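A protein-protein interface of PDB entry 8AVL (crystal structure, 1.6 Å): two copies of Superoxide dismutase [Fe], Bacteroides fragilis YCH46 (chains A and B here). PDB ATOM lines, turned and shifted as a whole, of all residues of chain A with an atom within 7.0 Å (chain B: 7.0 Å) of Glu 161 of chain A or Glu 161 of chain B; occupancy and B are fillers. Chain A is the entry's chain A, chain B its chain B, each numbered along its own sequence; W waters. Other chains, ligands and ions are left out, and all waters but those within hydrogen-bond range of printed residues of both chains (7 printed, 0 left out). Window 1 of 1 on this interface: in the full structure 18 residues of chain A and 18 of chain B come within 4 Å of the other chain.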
ATOM      1  N   HIS A  30      -8.765  14.187  22.022  1.00  0.00           N
ATOM      2  CA  HIS A  30      -9.931  13.329  21.752  1.00  0.00           C
ATOM      3  C   HIS A  30      -9.935  12.866  20.308  1.00  0.00           C
ATOM      4  O   HIS A  30     -10.022  11.669  20.056  1.00  0.00           O
ATOM      5  CB  HIS A  30     -11.261  14.000  22.139  1.00  0.00           C
ATOM      6  CG  HIS A  30     -11.445  14.149  23.620  1.00  0.00           C
ATOM      7  ND1 HIS A  30     -12.035  13.212  24.445  1.00  0.00           N
ATOM      8  CD2 HIS A  30     -11.069  15.187  24.435  1.00  0.00           C
ATOM      9  CE1 HIS A  30     -12.017  13.684  25.687  1.00  0.00           C
ATOM     10  NE2 HIS A  30     -11.443  14.880  25.710  1.00  0.00           N
ATOM     11  N   TYR A  34      -9.520   8.994  18.669  1.00  0.00           N
ATOM     12  CA  TYR A  34     -10.492   8.338  17.800  1.00  0.00           C
ATOM     13  C   TYR A  34      -9.829   7.891  16.496  1.00  0.00           C
ATOM     14  O   TYR A  34     -10.103   6.784  16.027  1.00  0.00           O
ATOM     15  CB  TYR A  34     -11.675   9.263  17.526  1.00  0.00           C
ATOM     16  CG  TYR A  34     -12.527   9.600  18.731  1.00  0.00           C
ATOM     17  CD1 TYR A  34     -13.046   8.596  19.555  1.00  0.00           C
ATOM     18  CD2 TYR A  34     -12.886  10.916  19.006  1.00  0.00           C
ATOM     19  CE1 TYR A  34     -13.863   8.897  20.630  1.00  0.00           C
ATOM     20  CE2 TYR A  34     -13.725  11.218  20.074  1.00  0.00           C
ATOM     21  CZ  TYR A  34     -14.226  10.208  20.884  1.00  0.00           C
ATOM     22  OH  TYR A  34     -15.066  10.543  21.922  1.00  0.00           O
ATOM     23  N   GLY A 121     -27.034  12.773  28.261  1.00  0.00           N
ATOM     24  CA  GLY A 121     -25.774  12.066  28.133  1.00  0.00           C
ATOM     25  C   GLY A 121     -24.926  12.670  27.016  1.00  0.00           C
ATOM     26  O   GLY A 121     -25.001  13.864  26.763  1.00  0.00           O
ATOM     27  N   SER A 122     -24.149  11.801  26.345  1.00  0.00           N
ATOM     28  CA  SER A 122     -23.238  12.182  25.305  1.00  0.00           C
ATOM     29  C   SER A 122     -23.946  12.030  23.965  1.00  0.00           C
ATOM     30  O   SER A 122     -24.671  11.069  23.751  1.00  0.00           O
ATOM     31  CB  SER A 122     -21.988  11.346  25.361  1.00  0.00           C
ATOM     32  OG  SER A 122     -21.302  11.463  26.598  1.00  0.00           O
ATOM     33  N   GLY A 123     -23.637  12.964  23.046  1.00  0.00           N
ATOM     34  CA  GLY A 123     -24.104  12.840  21.681  1.00  0.00           C
ATOM     35  C   GLY A 123     -23.930  14.113  20.890  1.00  0.00           C
ATOM     36  O   GLY A 123     -23.192  15.010  21.307  1.00  0.00           O
ATOM     37  N   ASP A 158     -21.599  19.271  19.061  1.00  0.00           N
ATOM     38  CA  ASP A 158     -21.099  18.273  19.977  1.00  0.00           C
ATOM     39  C   ASP A 158     -21.567  18.604  21.390  1.00  0.00           C
ATOM     40  O   ASP A 158     -21.196  19.664  21.907  1.00  0.00           O
ATOM     41  CB  ASP A 158     -19.576  18.274  19.968  1.00  0.00           C
ATOM     42  CG  ASP A 158     -18.937  17.094  20.658  1.00  0.00           C
ATOM     43  OD1 ASP A 158     -19.658  16.252  21.249  1.00  0.00           O
ATOM     44  OD2 ASP A 158     -17.705  17.008  20.559  1.00  0.00           O
ATOM     45  N   VAL A 159     -22.370  17.719  21.986  1.00  0.00           N
ATOM     46  CA  VAL A 159     -22.817  17.961  23.361  1.00  0.00           C
ATOM     47  C   VAL A 159     -22.259  16.898  24.337  1.00  0.00           C
ATOM     48  O   VAL A 159     -22.673  16.855  25.484  1.00  0.00           O
ATOM     49  CB  VAL A 159     -24.353  18.150  23.443  1.00  0.00           C
ATOM     50  CG1 VAL A 159     -24.775  19.376  22.697  1.00  0.00           C
ATOM     51  CG2 VAL A 159     -25.168  16.952  23.005  1.00  0.00           C
ATOM     52  N   TRP A 160     -21.254  16.125  23.908  1.00  0.00           N
ATOM     53  CA  TRP A 160     -20.349  15.509  24.867  1.00  0.00           C
ATOM     54  C   TRP A 160     -19.775  16.596  25.770  1.00  0.00           C
ATOM     55  O   TRP A 160     -19.398  17.674  25.312  1.00  0.00           O
ATOM     56  CB  TRP A 160     -19.197  14.748  24.191  1.00  0.00           C
ATOM     57  CG  TRP A 160     -19.560  13.505  23.441  1.00  0.00           C
ATOM     58  CD1 TRP A 160     -20.414  13.358  22.387  1.00  0.00           C
ATOM     59  CD2 TRP A 160     -18.990  12.208  23.680  1.00  0.00           C
ATOM     60  NE1 TRP A 160     -20.419  12.058  21.956  1.00  0.00           N
ATOM     61  CE2 TRP A 160     -19.562  11.319  22.738  1.00  0.00           C
ATOM     62  CE3 TRP A 160     -18.080  11.703  24.618  1.00  0.00           C
ATOM     63  CZ2 TRP A 160     -19.234   9.959  22.708  1.00  0.00           C
ATOM     64  CZ3 TRP A 160     -17.774  10.350  24.598  1.00  0.00           C
ATOM     65  CH2 TRP A 160     -18.317   9.500  23.627  1.00  0.00           C
ATOM     66  N   GLU A 161     -19.675  16.285  27.063  1.00  0.00           N
ATOM     67  CA  GLU A 161     -19.182  17.265  28.032  1.00  0.00           C
ATOM     68  C   GLU A 161     -17.789  17.793  27.687  1.00  0.00           C
ATOM     69  O   GLU A 161     -17.524  18.955  27.933  1.00  0.00           O
ATOM     70  CB  GLU A 161     -19.270  16.701  29.453  1.00  0.00           C
ATOM     71  CG  GLU A 161     -20.702  16.664  29.950  1.00  0.00           C
ATOM     72  CD  GLU A 161     -20.927  16.012  31.315  1.00  0.00           C
ATOM     73  OE1 GLU A 161     -20.313  14.955  31.606  1.00  0.00           O
ATOM     74  OE2 GLU A 161     -21.747  16.546  32.077  1.00  0.00           O
ATOM     75  N   HIS A 162     -16.923  16.989  27.091  1.00  0.00           N
ATOM     76  CA  HIS A 162     -15.580  17.457  26.758  1.00  0.00           C
ATOM     77  C   HIS A 162     -15.597  18.648  25.796  1.00  0.00           C
ATOM     78  O   HIS A 162     -14.615  19.396  25.756  1.00  0.00           O
ATOM     79  CB  HIS A 162     -14.663  16.339  26.251  1.00  0.00           C
ATOM     80  CG  HIS A 162     -15.075  15.703  24.974  1.00  0.00           C
ATOM     81  ND1 HIS A 162     -15.297  14.355  24.892  1.00  0.00           N
ATOM     82  CD2 HIS A 162     -15.283  16.177  23.745  1.00  0.00           C
ATOM     83  CE1 HIS A 162     -15.658  14.049  23.668  1.00  0.00           C
ATOM     84  NE2 HIS A 162     -15.633  15.118  22.941  1.00  0.00           N
ATOM     85  N   ALA A 163     -16.689  18.835  25.033  1.00  0.00           N
ATOM     86  CA  ALA A 163     -16.766  19.923  24.068  1.00  0.00           C
ATOM     87  C   ALA A 163     -16.829  21.290  24.749  1.00  0.00           C
ATOM     88  O   ALA A 163     -16.473  22.296  24.124  1.00  0.00           O
ATOM     89  CB  ALA A 163     -17.966  19.759  23.148  1.00  0.00           C
ATOM     90  N   TYR A 164     -17.304  21.320  26.012  1.00  0.00           N
ATOM     91  CA  TYR A 164     -17.604  22.575  26.678  1.00  0.00           C
ATOM     92  C   TYR A 164     -17.196  22.624  28.149  1.00  0.00           C
ATOM     93  O   TYR A 164     -17.180  23.720  28.707  1.00  0.00           O
ATOM     94  CB  TYR A 164     -19.091  22.907  26.539  1.00  0.00           C
ATOM     95  CG  TYR A 164     -20.073  21.893  27.096  1.00  0.00           C
ATOM     96  CD1 TYR A 164     -20.436  21.879  28.435  1.00  0.00           C
ATOM     97  CD2 TYR A 164     -20.664  20.943  26.264  1.00  0.00           C
ATOM     98  CE1 TYR A 164     -21.370  20.968  28.926  1.00  0.00           C
ATOM     99  CE2 TYR A 164     -21.599  20.045  26.738  1.00  0.00           C
ATOM    100  CZ  TYR A 164     -21.953  20.044  28.075  1.00  0.00           C
ATOM    101  OH  TYR A 164     -22.868  19.151  28.539  1.00  0.00           O
ATOM    102  N   TYR A 165     -16.821  21.503  28.780  1.00  0.00           N
ATOM    103  CA  TYR A 165     -16.744  21.471  30.242  1.00  0.00           C
ATOM    104  C   TYR A 165     -15.661  22.420  30.778  1.00  0.00           C
ATOM    105  O   TYR A 165     -15.814  23.002  31.852  1.00  0.00           O
ATOM    106  CB  TYR A 165     -16.535  20.044  30.794  1.00  0.00           C
ATOM    107  CG  TYR A 165     -17.211  19.896  32.131  1.00  0.00           C
ATOM    108  CD1 TYR A 165     -18.592  19.764  32.215  1.00  0.00           C
ATOM    109  CD2 TYR A 165     -16.508  20.039  33.309  1.00  0.00           C
ATOM    110  CE1 TYR A 165     -19.247  19.704  33.434  1.00  0.00           C
ATOM    111  CE2 TYR A 165     -17.143  19.988  34.542  1.00  0.00           C
ATOM    112  CZ  TYR A 165     -18.524  19.855  34.606  1.00  0.00           C
ATOM    113  OH  TYR A 165     -19.159  19.857  35.819  1.00  0.00           O
ATOM    114  N   LEU A 166     -14.536  22.562  30.054  1.00  0.00           N
ATOM    115  CA  LEU A 166     -13.461  23.389  30.568  1.00  0.00           C
ATOM    116  C   LEU A 166     -13.855  24.870  30.597  1.00  0.00           C
ATOM    117  O   LEU A 166     -13.276  25.634  31.365  1.00  0.00           O
ATOM    118  CB  LEU A 166     -12.197  23.173  29.731  1.00  0.00           C
ATOM    119  CG  LEU A 166     -11.594  21.771  29.799  1.00  0.00           C
ATOM    120  CD1 LEU A 166     -10.426  21.708  28.832  1.00  0.00           C
ATOM    121  CD2 LEU A 166     -11.175  21.386  31.221  1.00  0.00           C
ATOM    122  N   GLN A 169     -18.423  24.375  32.121  1.00  0.00           N
ATOM    123  CA  GLN A 169     -18.810  23.335  33.075  1.00  0.00           C
ATOM    124  C   GLN A 169     -20.195  22.775  32.703  1.00  0.00           C
ATOM    125  O   GLN A 169     -20.407  22.351  31.583  1.00  0.00           O
ATOM    126  CB  GLN A 169     -18.625  23.845  34.519  1.00  0.00           C
ATOM    127  CG  GLN A 169     -17.195  24.223  34.845  1.00  0.00           C
ATOM    128  CD  GLN A 169     -16.725  25.545  34.279  1.00  0.00           C
ATOM    129  OE1 GLN A 169     -17.395  26.553  34.468  1.00  0.00           O
ATOM    130  NE2 GLN A 169     -15.590  25.538  33.570  1.00  0.00           N
ATOM    131  N   ASN A 170     -21.124  22.743  33.657  1.00  0.00           N
ATOM    132  CA  ASN A 170     -22.451  22.138  33.483  1.00  0.00           C
ATOM    133  C   ASN A 170     -23.373  22.949  32.561  1.00  0.00           C
ATOM    134  O   ASN A 170     -24.455  22.464  32.240  1.00  0.00           O
ATOM    135  CB  ASN A 170     -23.136  21.968  34.850  1.00  0.00           C
ATOM    136  CG  ASN A 170     -23.334  23.270  35.588  1.00  0.00           C
ATOM    137  OD1 ASN A 170     -22.357  23.944  35.909  1.00  0.00           O
ATOM    138  ND2 ASN A 170     -24.576  23.617  35.873  1.00  0.00           N
ATOM    139  N   ARG A 172     -24.379  23.723  29.572  1.00  0.00           N
ATOM    140  CA  ARG A 172     -24.387  23.354  28.164  1.00  0.00           C
ATOM    141  C   ARG A 172     -25.135  24.395  27.323  1.00  0.00           C
ATOM    142  O   ARG A 172     -24.686  24.758  26.239  1.00  0.00           O
ATOM    143  CB  ARG A 172     -25.061  21.980  27.979  1.00  0.00           C
ATOM    144  CG  ARG A 172     -24.999  21.493  26.523  1.00  0.00           C
ATOM    145  CD  ARG A 172     -25.894  20.312  26.258  1.00  0.00           C
ATOM    146  NE  ARG A 172     -25.424  19.072  26.852  1.00  0.00           N
ATOM    147  CZ  ARG A 172     -26.089  17.918  26.721  1.00  0.00           C
ATOM    148  NH1 ARG A 172     -27.195  17.855  25.968  1.00  0.00           N
ATOM    149  NH2 ARG A 172     -25.648  16.841  27.321  1.00  0.00           N
ATOM    150  N   HIS B  30     -24.418  19.527  39.357  1.00  0.00           N
ATOM    151  CA  HIS B  30     -25.046  18.430  38.611  1.00  0.00           C
ATOM    152  C   HIS B  30     -26.084  17.702  39.478  1.00  0.00           C
ATOM    153  O   HIS B  30     -27.204  17.521  39.063  1.00  0.00           O
ATOM    154  CB  HIS B  30     -24.015  17.429  38.058  1.00  0.00           C
ATOM    155  CG  HIS B  30     -23.192  18.008  36.954  1.00  0.00           C
ATOM    156  ND1 HIS B  30     -23.507  17.905  35.616  1.00  0.00           N
ATOM    157  CD2 HIS B  30     -22.010  18.645  37.027  1.00  0.00           C
ATOM    158  CE1 HIS B  30     -22.539  18.485  34.907  1.00  0.00           C
ATOM    159  NE2 HIS B  30     -21.640  18.960  35.747  1.00  0.00           N
ATOM    160  N   TYR B  34     -30.220  17.405  39.014  1.00  0.00           N
ATOM    161  CA  TYR B  34     -30.972  16.142  38.927  1.00  0.00           C
ATOM    162  C   TYR B  34     -32.090  16.108  39.954  1.00  0.00           C
ATOM    163  O   TYR B  34     -33.193  15.688  39.604  1.00  0.00           O
ATOM    164  CB  TYR B  34     -30.059  14.930  39.106  1.00  0.00           C
ATOM    165  CG  TYR B  34     -29.046  14.748  37.995  1.00  0.00           C
ATOM    166  CD1 TYR B  34     -29.411  14.772  36.651  1.00  0.00           C
ATOM    167  CD2 TYR B  34     -27.710  14.509  38.279  1.00  0.00           C
ATOM    168  CE1 TYR B  34     -28.490  14.537  35.636  1.00  0.00           C
ATOM    169  CE2 TYR B  34     -26.784  14.279  37.274  1.00  0.00           C
ATOM    170  CZ  TYR B  34     -27.175  14.298  35.955  1.00  0.00           C
ATOM    171  OH  TYR B  34     -26.263  14.042  34.974  1.00  0.00           O
ATOM    172  N   GLY B 121     -19.105   6.700  25.909  1.00  0.00           N
ATOM    173  CA  GLY B 121     -20.084   7.729  26.213  1.00  0.00           C
ATOM    174  C   GLY B 121     -20.142   7.951  27.724  1.00  0.00           C
ATOM    175  O   GLY B 121     -19.160   7.726  28.470  1.00  0.00           O
ATOM    176  N   SER B 122     -21.339   8.371  28.148  1.00  0.00           N
ATOM    177  CA  SER B 122     -21.636   8.666  29.548  1.00  0.00           C
ATOM    178  C   SER B 122     -22.201   7.405  30.187  1.00  0.00           C
ATOM    179  O   SER B 122     -22.956   6.673  29.553  1.00  0.00           O
ATOM    180  CB  SER B 122     -22.619   9.786  29.683  1.00  0.00           C
ATOM    181  OG  SER B 122     -22.163  10.989  29.058  1.00  0.00           O
ATOM    182  N   GLY B 123     -21.846   7.183  31.455  1.00  0.00           N
ATOM    183  CA  GLY B 123     -22.472   6.116  32.209  1.00  0.00           C
ATOM    184  C   GLY B 123     -21.729   5.828  33.491  1.00  0.00           C
ATOM    185  O   GLY B 123     -20.928   6.627  33.961  1.00  0.00           O
ATOM    186  N   ASP B 158     -18.582   6.698  38.488  1.00  0.00           N
ATOM    187  CA  ASP B 158     -19.164   7.606  37.529  1.00  0.00           C
ATOM    188  C   ASP B 158     -18.139   7.910  36.449  1.00  0.00           C
ATOM    189  O   ASP B 158     -17.071   8.462  36.772  1.00  0.00           O
ATOM    190  CB  ASP B 158     -19.530   8.917  38.220  1.00  0.00           C
ATOM    191  CG  ASP B 158     -20.397   9.840  37.410  1.00  0.00           C
ATOM    192  OD1 ASP B 158     -20.707   9.535  36.227  1.00  0.00           O
ATOM    193  OD2 ASP B 158     -20.762  10.837  37.989  1.00  0.00           O
ATOM    194  N   VAL B 159     -18.442   7.558  35.200  1.00  0.00           N
ATOM    195  CA  VAL B 159     -17.519   7.854  34.115  1.00  0.00           C
ATOM    196  C   VAL B 159     -18.131   8.833  33.101  1.00  0.00           C
ATOM    197  O   VAL B 159     -17.586   9.034  32.003  1.00  0.00           O
ATOM    198  CB  VAL B 159     -16.957   6.566  33.461  1.00  0.00           C
ATOM    199  CG1 VAL B 159     -16.099   5.791  34.458  1.00  0.00           C
ATOM    200  CG2 VAL B 159     -18.009   5.644  32.858  1.00  0.00           C
ATOM    201  N   TRP B 160     -19.227   9.523  33.486  1.00  0.00           N
ATOM    202  CA  TRP B 160     -19.546  10.787  32.843  1.00  0.00           C
ATOM    203  C   TRP B 160     -18.336  11.703  32.947  1.00  0.00           C
ATOM    204  O   TRP B 160     -17.662  11.752  33.965  1.00  0.00           O
ATOM    205  CB  TRP B 160     -20.748  11.482  33.482  1.00  0.00           C
ATOM    206  CG  TRP B 160     -22.091  10.863  33.266  1.00  0.00           C
ATOM    207  CD1 TRP B 160     -22.506   9.618  33.620  1.00  0.00           C
ATOM    208  CD2 TRP B 160     -23.229  11.529  32.691  1.00  0.00           C
ATOM    209  NE1 TRP B 160     -23.824   9.459  33.292  1.00  0.00           N
ATOM    210  CE2 TRP B 160     -24.304  10.621  32.735  1.00  0.00           C
ATOM    211  CE3 TRP B 160     -23.439  12.796  32.117  1.00  0.00           C
ATOM    212  CZ2 TRP B 160     -25.566  10.950  32.247  1.00  0.00           C
ATOM    213  CZ3 TRP B 160     -24.697  13.131  31.657  1.00  0.00           C
ATOM    214  CH2 TRP B 160     -25.739  12.215  31.720  1.00  0.00           C
ATOM    215  N   GLU B 161     -18.054  12.431  31.866  1.00  0.00           N
ATOM    216  CA  GLU B 161     -16.881  13.298  31.832  1.00  0.00           C
ATOM    217  C   GLU B 161     -16.865  14.327  32.968  1.00  0.00           C
ATOM    218  O   GLU B 161     -15.797  14.622  33.493  1.00  0.00           O
ATOM    219  CB  GLU B 161     -16.719  13.918  30.452  1.00  0.00           C
ATOM    220  CG  GLU B 161     -16.303  12.889  29.417  1.00  0.00           C
ATOM    221  CD  GLU B 161     -16.160  13.371  27.989  1.00  0.00           C
ATOM    222  OE1 GLU B 161     -17.064  14.157  27.536  1.00  0.00           O
ATOM    223  OE2 GLU B 161     -15.126  12.998  27.344  1.00  0.00           O
ATOM    224  N   HIS B 162     -18.028  14.836  33.392  1.00  0.00           N
ATOM    225  CA  HIS B 162     -18.070  15.779  34.482  1.00  0.00           C
ATOM    226  C   HIS B 162     -17.461  15.249  35.783  1.00  0.00           C
ATOM    227  O   HIS B 162     -17.048  16.064  36.617  1.00  0.00           O
ATOM    228  CB  HIS B 162     -19.472  16.328  34.709  1.00  0.00           C
ATOM    229  CG  HIS B 162     -20.498  15.359  35.161  1.00  0.00           C
ATOM    230  ND1 HIS B 162     -21.663  15.209  34.465  1.00  0.00           N
ATOM    231  CD2 HIS B 162     -20.582  14.563  36.240  1.00  0.00           C
ATOM    232  CE1 HIS B 162     -22.415  14.311  35.110  1.00  0.00           C
ATOM    233  NE2 HIS B 162     -21.782  13.889  36.180  1.00  0.00           N
ATOM    234  N   ALA B 163     -17.395  13.928  35.966  1.00  0.00           N
ATOM    235  CA  ALA B 163     -16.865  13.334  37.196  1.00  0.00           C
ATOM    236  C   ALA B 163     -15.360  13.550  37.314  1.00  0.00           C
ATOM    237  O   ALA B 163     -14.842  13.479  38.424  1.00  0.00           O
ATOM    238  CB  ALA B 163     -17.184  11.853  37.256  1.00  0.00           C
ATOM    239  N   TYR B 164     -14.660  13.785  36.188  1.00  0.00           N
ATOM    240  CA  TYR B 164     -13.208  13.819  36.183  1.00  0.00           C
ATOM    241  C   TYR B 164     -12.580  14.904  35.296  1.00  0.00           C
ATOM    242  O   TYR B 164     -11.365  15.136  35.393  1.00  0.00           O
ATOM    243  CB  TYR B 164     -12.640  12.442  35.800  1.00  0.00           C
ATOM    244  CG  TYR B 164     -13.039  11.906  34.440  1.00  0.00           C
ATOM    245  CD1 TYR B 164     -12.348  12.256  33.276  1.00  0.00           C
ATOM    246  CD2 TYR B 164     -14.105  11.035  34.304  1.00  0.00           C
ATOM    247  CE1 TYR B 164     -12.720  11.772  32.027  1.00  0.00           C
ATOM    248  CE2 TYR B 164     -14.487  10.543  33.064  1.00  0.00           C
ATOM    249  CZ  TYR B 164     -13.781  10.891  31.923  1.00  0.00           C
ATOM    250  OH  TYR B 164     -14.169  10.349  30.723  1.00  0.00           O
ATOM    251  N   TYR B 165     -13.351  15.556  34.422  1.00  0.00           N
ATOM    252  CA  TYR B 165     -12.746  16.326  33.329  1.00  0.00           C
ATOM    253  C   TYR B 165     -11.934  17.524  33.855  1.00  0.00           C
ATOM    254  O   TYR B 165     -10.915  17.900  33.263  1.00  0.00           O
ATOM    255  CB  TYR B 165     -13.799  16.812  32.306  1.00  0.00           C
ATOM    256  CG  TYR B 165     -13.199  16.870  30.927  1.00  0.00           C
ATOM    257  CD1 TYR B 165     -12.964  15.705  30.184  1.00  0.00           C
ATOM    258  CD2 TYR B 165     -12.734  18.062  30.408  1.00  0.00           C
ATOM    259  CE1 TYR B 165     -12.354  15.756  28.937  1.00  0.00           C
ATOM    260  CE2 TYR B 165     -12.111  18.125  29.175  1.00  0.00           C
ATOM    261  CZ  TYR B 165     -11.892  16.969  28.449  1.00  0.00           C
ATOM    262  OH  TYR B 165     -11.239  17.004  27.251  1.00  0.00           O
ATOM    263  N   LEU B 166     -12.354  18.147  34.955  1.00  0.00           N
ATOM    264  CA  LEU B 166     -11.636  19.310  35.463  1.00  0.00           C
ATOM    265  C   LEU B 166     -10.248  18.925  35.994  1.00  0.00           C
ATOM    266  O   LEU B 166      -9.359  19.774  36.024  1.00  0.00           O
ATOM    267  CB  LEU B 166     -12.451  19.999  36.557  1.00  0.00           C
ATOM    268  CG  LEU B 166     -13.779  20.608  36.106  1.00  0.00           C
ATOM    269  CD1 LEU B 166     -14.589  21.058  37.328  1.00  0.00           C
ATOM    270  CD2 LEU B 166     -13.556  21.733  35.124  1.00  0.00           C
ATOM    271  N   GLN B 169      -9.024  15.741  32.557  1.00  0.00           N
ATOM    272  CA  GLN B 169      -9.415  15.921  31.161  1.00  0.00           C
ATOM    273  C   GLN B 169      -9.742  14.554  30.548  1.00  0.00           C
ATOM    274  O   GLN B 169     -10.553  13.827  31.108  1.00  0.00           O
ATOM    275  CB  GLN B 169      -8.394  16.787  30.416  1.00  0.00           C
ATOM    276  CG  GLN B 169      -8.231  18.195  30.997  1.00  0.00           C
ATOM    277  CD  GLN B 169      -7.426  18.260  32.274  1.00  0.00           C
ATOM    278  OE1 GLN B 169      -6.313  17.735  32.336  1.00  0.00           O
ATOM    279  NE2 GLN B 169      -7.983  18.899  33.294  1.00  0.00           N
ATOM    280  N   ASN B 170      -9.139  14.220  29.399  1.00  0.00           N
ATOM    281  CA  ASN B 170      -9.435  12.991  28.660  1.00  0.00           C
ATOM    282  C   ASN B 170      -8.922  11.720  29.349  1.00  0.00           C
ATOM    283  O   ASN B 170      -9.218  10.624  28.881  1.00  0.00           O
ATOM    284  CB  ASN B 170      -8.849  13.047  27.243  1.00  0.00           C
ATOM    285  CG  ASN B 170      -7.352  13.241  27.216  1.00  0.00           C
ATOM    286  OD1 ASN B 170      -6.832  14.194  27.762  1.00  0.00           O
ATOM    287  ND2 ASN B 170      -6.647  12.309  26.606  1.00  0.00           N
ATOM    288  N   ARG B 172      -9.343   9.386  31.561  1.00  0.00           N
ATOM    289  CA  ARG B 172     -10.306   8.713  32.424  1.00  0.00           C
ATOM    290  C   ARG B 172      -9.618   7.652  33.290  1.00  0.00           C
ATOM    291  O   ARG B 172      -9.901   7.534  34.484  1.00  0.00           O
ATOM    292  CB  ARG B 172     -11.438   8.104  31.594  1.00  0.00           C
ATOM    293  CG  ARG B 172     -12.509   7.472  32.471  1.00  0.00           C
ATOM    294  CD  ARG B 172     -13.489   6.594  31.740  1.00  0.00           C
ATOM    295  NE  ARG B 172     -14.416   7.309  30.876  1.00  0.00           N
ATOM    296  CZ  ARG B 172     -15.325   6.713  30.106  1.00  0.00           C
ATOM    297  NH1 ARG B 172     -15.473   5.414  30.177  1.00  0.00           N
ATOM    298  NH2 ARG B 172     -16.071   7.412  29.271  1.00  0.00           N
HETATM  299  O   HOH W   1     -18.251  18.235  38.000  1.00  0.00           O
HETATM  300  O   HOH W   2     -11.882  18.892  25.245  1.00  0.00           O
HETATM  301  O   HOH W   3     -24.555  16.602  33.381  1.00  0.00           O
HETATM  302  O   HOH W   4     -23.796   8.930  26.668  1.00  0.00           O
HETATM  303  O   HOH W   5     -13.953  11.281  25.138  1.00  0.00           O
HETATM  304  O   HOH W   6     -20.316  12.710  30.085  1.00  0.00           O
HETATM  305  O   HOH W   7     -19.724  13.451  27.508  1.00  0.00           O
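His 30 of chain A touches Tyr 165 of chain B, and with the chains exchanged Tyr 165 of chain A touches His 30 of chain B. Tyr 165 of chain A touches Leu 166 of chain B, and with the chains exchanged Leu 166 of chain A touches Tyr 165 of chain B.
Among the printed residues, merely in contact across the chains: Asn 170 of chain A with His 30 of chain B (3.5 Å), Glu 161 of chain A with His 30 of chain B (3.5 Å), His 30 of chain A with Asn 170 of chain B (3.5 Å), His 30 of chain A with Glu 161 of chain B (3.6 Å), His 162 of chain A with Tyr 165 of chain B (3.6 Å), Gly 121 of chain A with Trp 160 of chain B (3.6 Å), Trp 160 of chain A with Gly 121 of chain B (3.6 Å), Tyr 165 of chain A with His 162 of chain B (3.6 Å), Leu 166 of chain A with Tyr 165 of chain B (3.7 Å), Tyr 165 of chain A with Leu 166 of chain B (3.8 Å), Gly 121 of chain A with Ser 122 of chain B (3.8 Å), Glu 161 of chain A with Trp 160 of chain B (3.8 Å), Ser 122 of chain A with Gly 121 of chain B (3.9 Å) and Trp 160 of chain A with Glu 161 of chain B (3.9 Å).
Water W4 bridges the backbone NH of Ser 122 of chain A and the backbone NH of Ser 122 of chain B.
Of the printed residues of chain B, Trp 160 of chain A touches Gly 121 and Glu 161. Of chain B, only His 30 (3.5 Å), Trp 160 (3.8 Å), Glu 161 (3.4 Å) and His 162 (2.7 Å) come within 4 Å of Glu 161 of chain A. Printed residues of chain B within 4 Å of His 162 of chain A: Glu 161 and Tyr 165. Tyr 164 of chain A touches none of the printed residues of chain B. Glu 161 of chain B touches four residues of chain A. The nearest residue of chain A that does not touch Glu 161 of chain B is Ser 122 of chain A (5.1 Å). The nearest printed residue of chain B that does not touch Leu 166 of chain A is Gln 169 of chain B (4.3 Å).
The backbone carbonyl oxygen of Gly 121 of chain B is in hydrogen-bond range of the guanidinium group of Arg 172 of chain B, at 3.2 Å. The backbone carbonyl oxygen (O) of Leu 166 of chain B is in hydrogen-bond range of the side-chain amide nitrogen (NE2) of Gln 169 of chain B (3.2 Å).
A ring nitrogen (NE2) of His 30 of chain A is in hydrogen-bond range of the side-chain hydroxyl (OH) of Tyr 165 of chain B, at 2.6 Å. OG of Ser 122 of chain A is in hydrogen-bond range of OG of Ser 122 of chain B (2.6 Å). The side-chain carboxylate (OE1) of Glu 161 of chain A sits at hydrogen-bond distance from the backbone NH (N) of Glu 161 of chain B, at 3.4 Å. ND1 of His 162 of chain B lies within hydrogen-bond range of OE2 of Glu 161 of chain A. A ring nitrogen (ND1) of His 162 of chain A is in hydrogen-bond range of the side-chain carboxylate (OE2) of Glu 161 of chain B (2.8 Å). A ring nitrogen (NE2) of His 30 of chain B sits at hydrogen-bond distance from the side-chain hydroxyl (OH) of Tyr 165 of chain A (2.6 Å).
Hydrophobic or aromatic side chains of chain B that line the printed part of chain A: His 30, Trp 160, His 162, Tyr 165 and Leu 166. Of the 17 printed residues of chain A, 9 touch a printed residue of chain B. Hydrophobic or aromatic side chains of chain A within 4 Å of the printed part of chain B: His 30, Trp 160, His 162, Tyr 165 and Leu 166. Among the printed residues, 20 pairs touch across the chains. Among the printed residues, no Asp or Glu carboxylate lies within 4 Å of a Lys or Arg side-chain nitrogen of the other chain.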
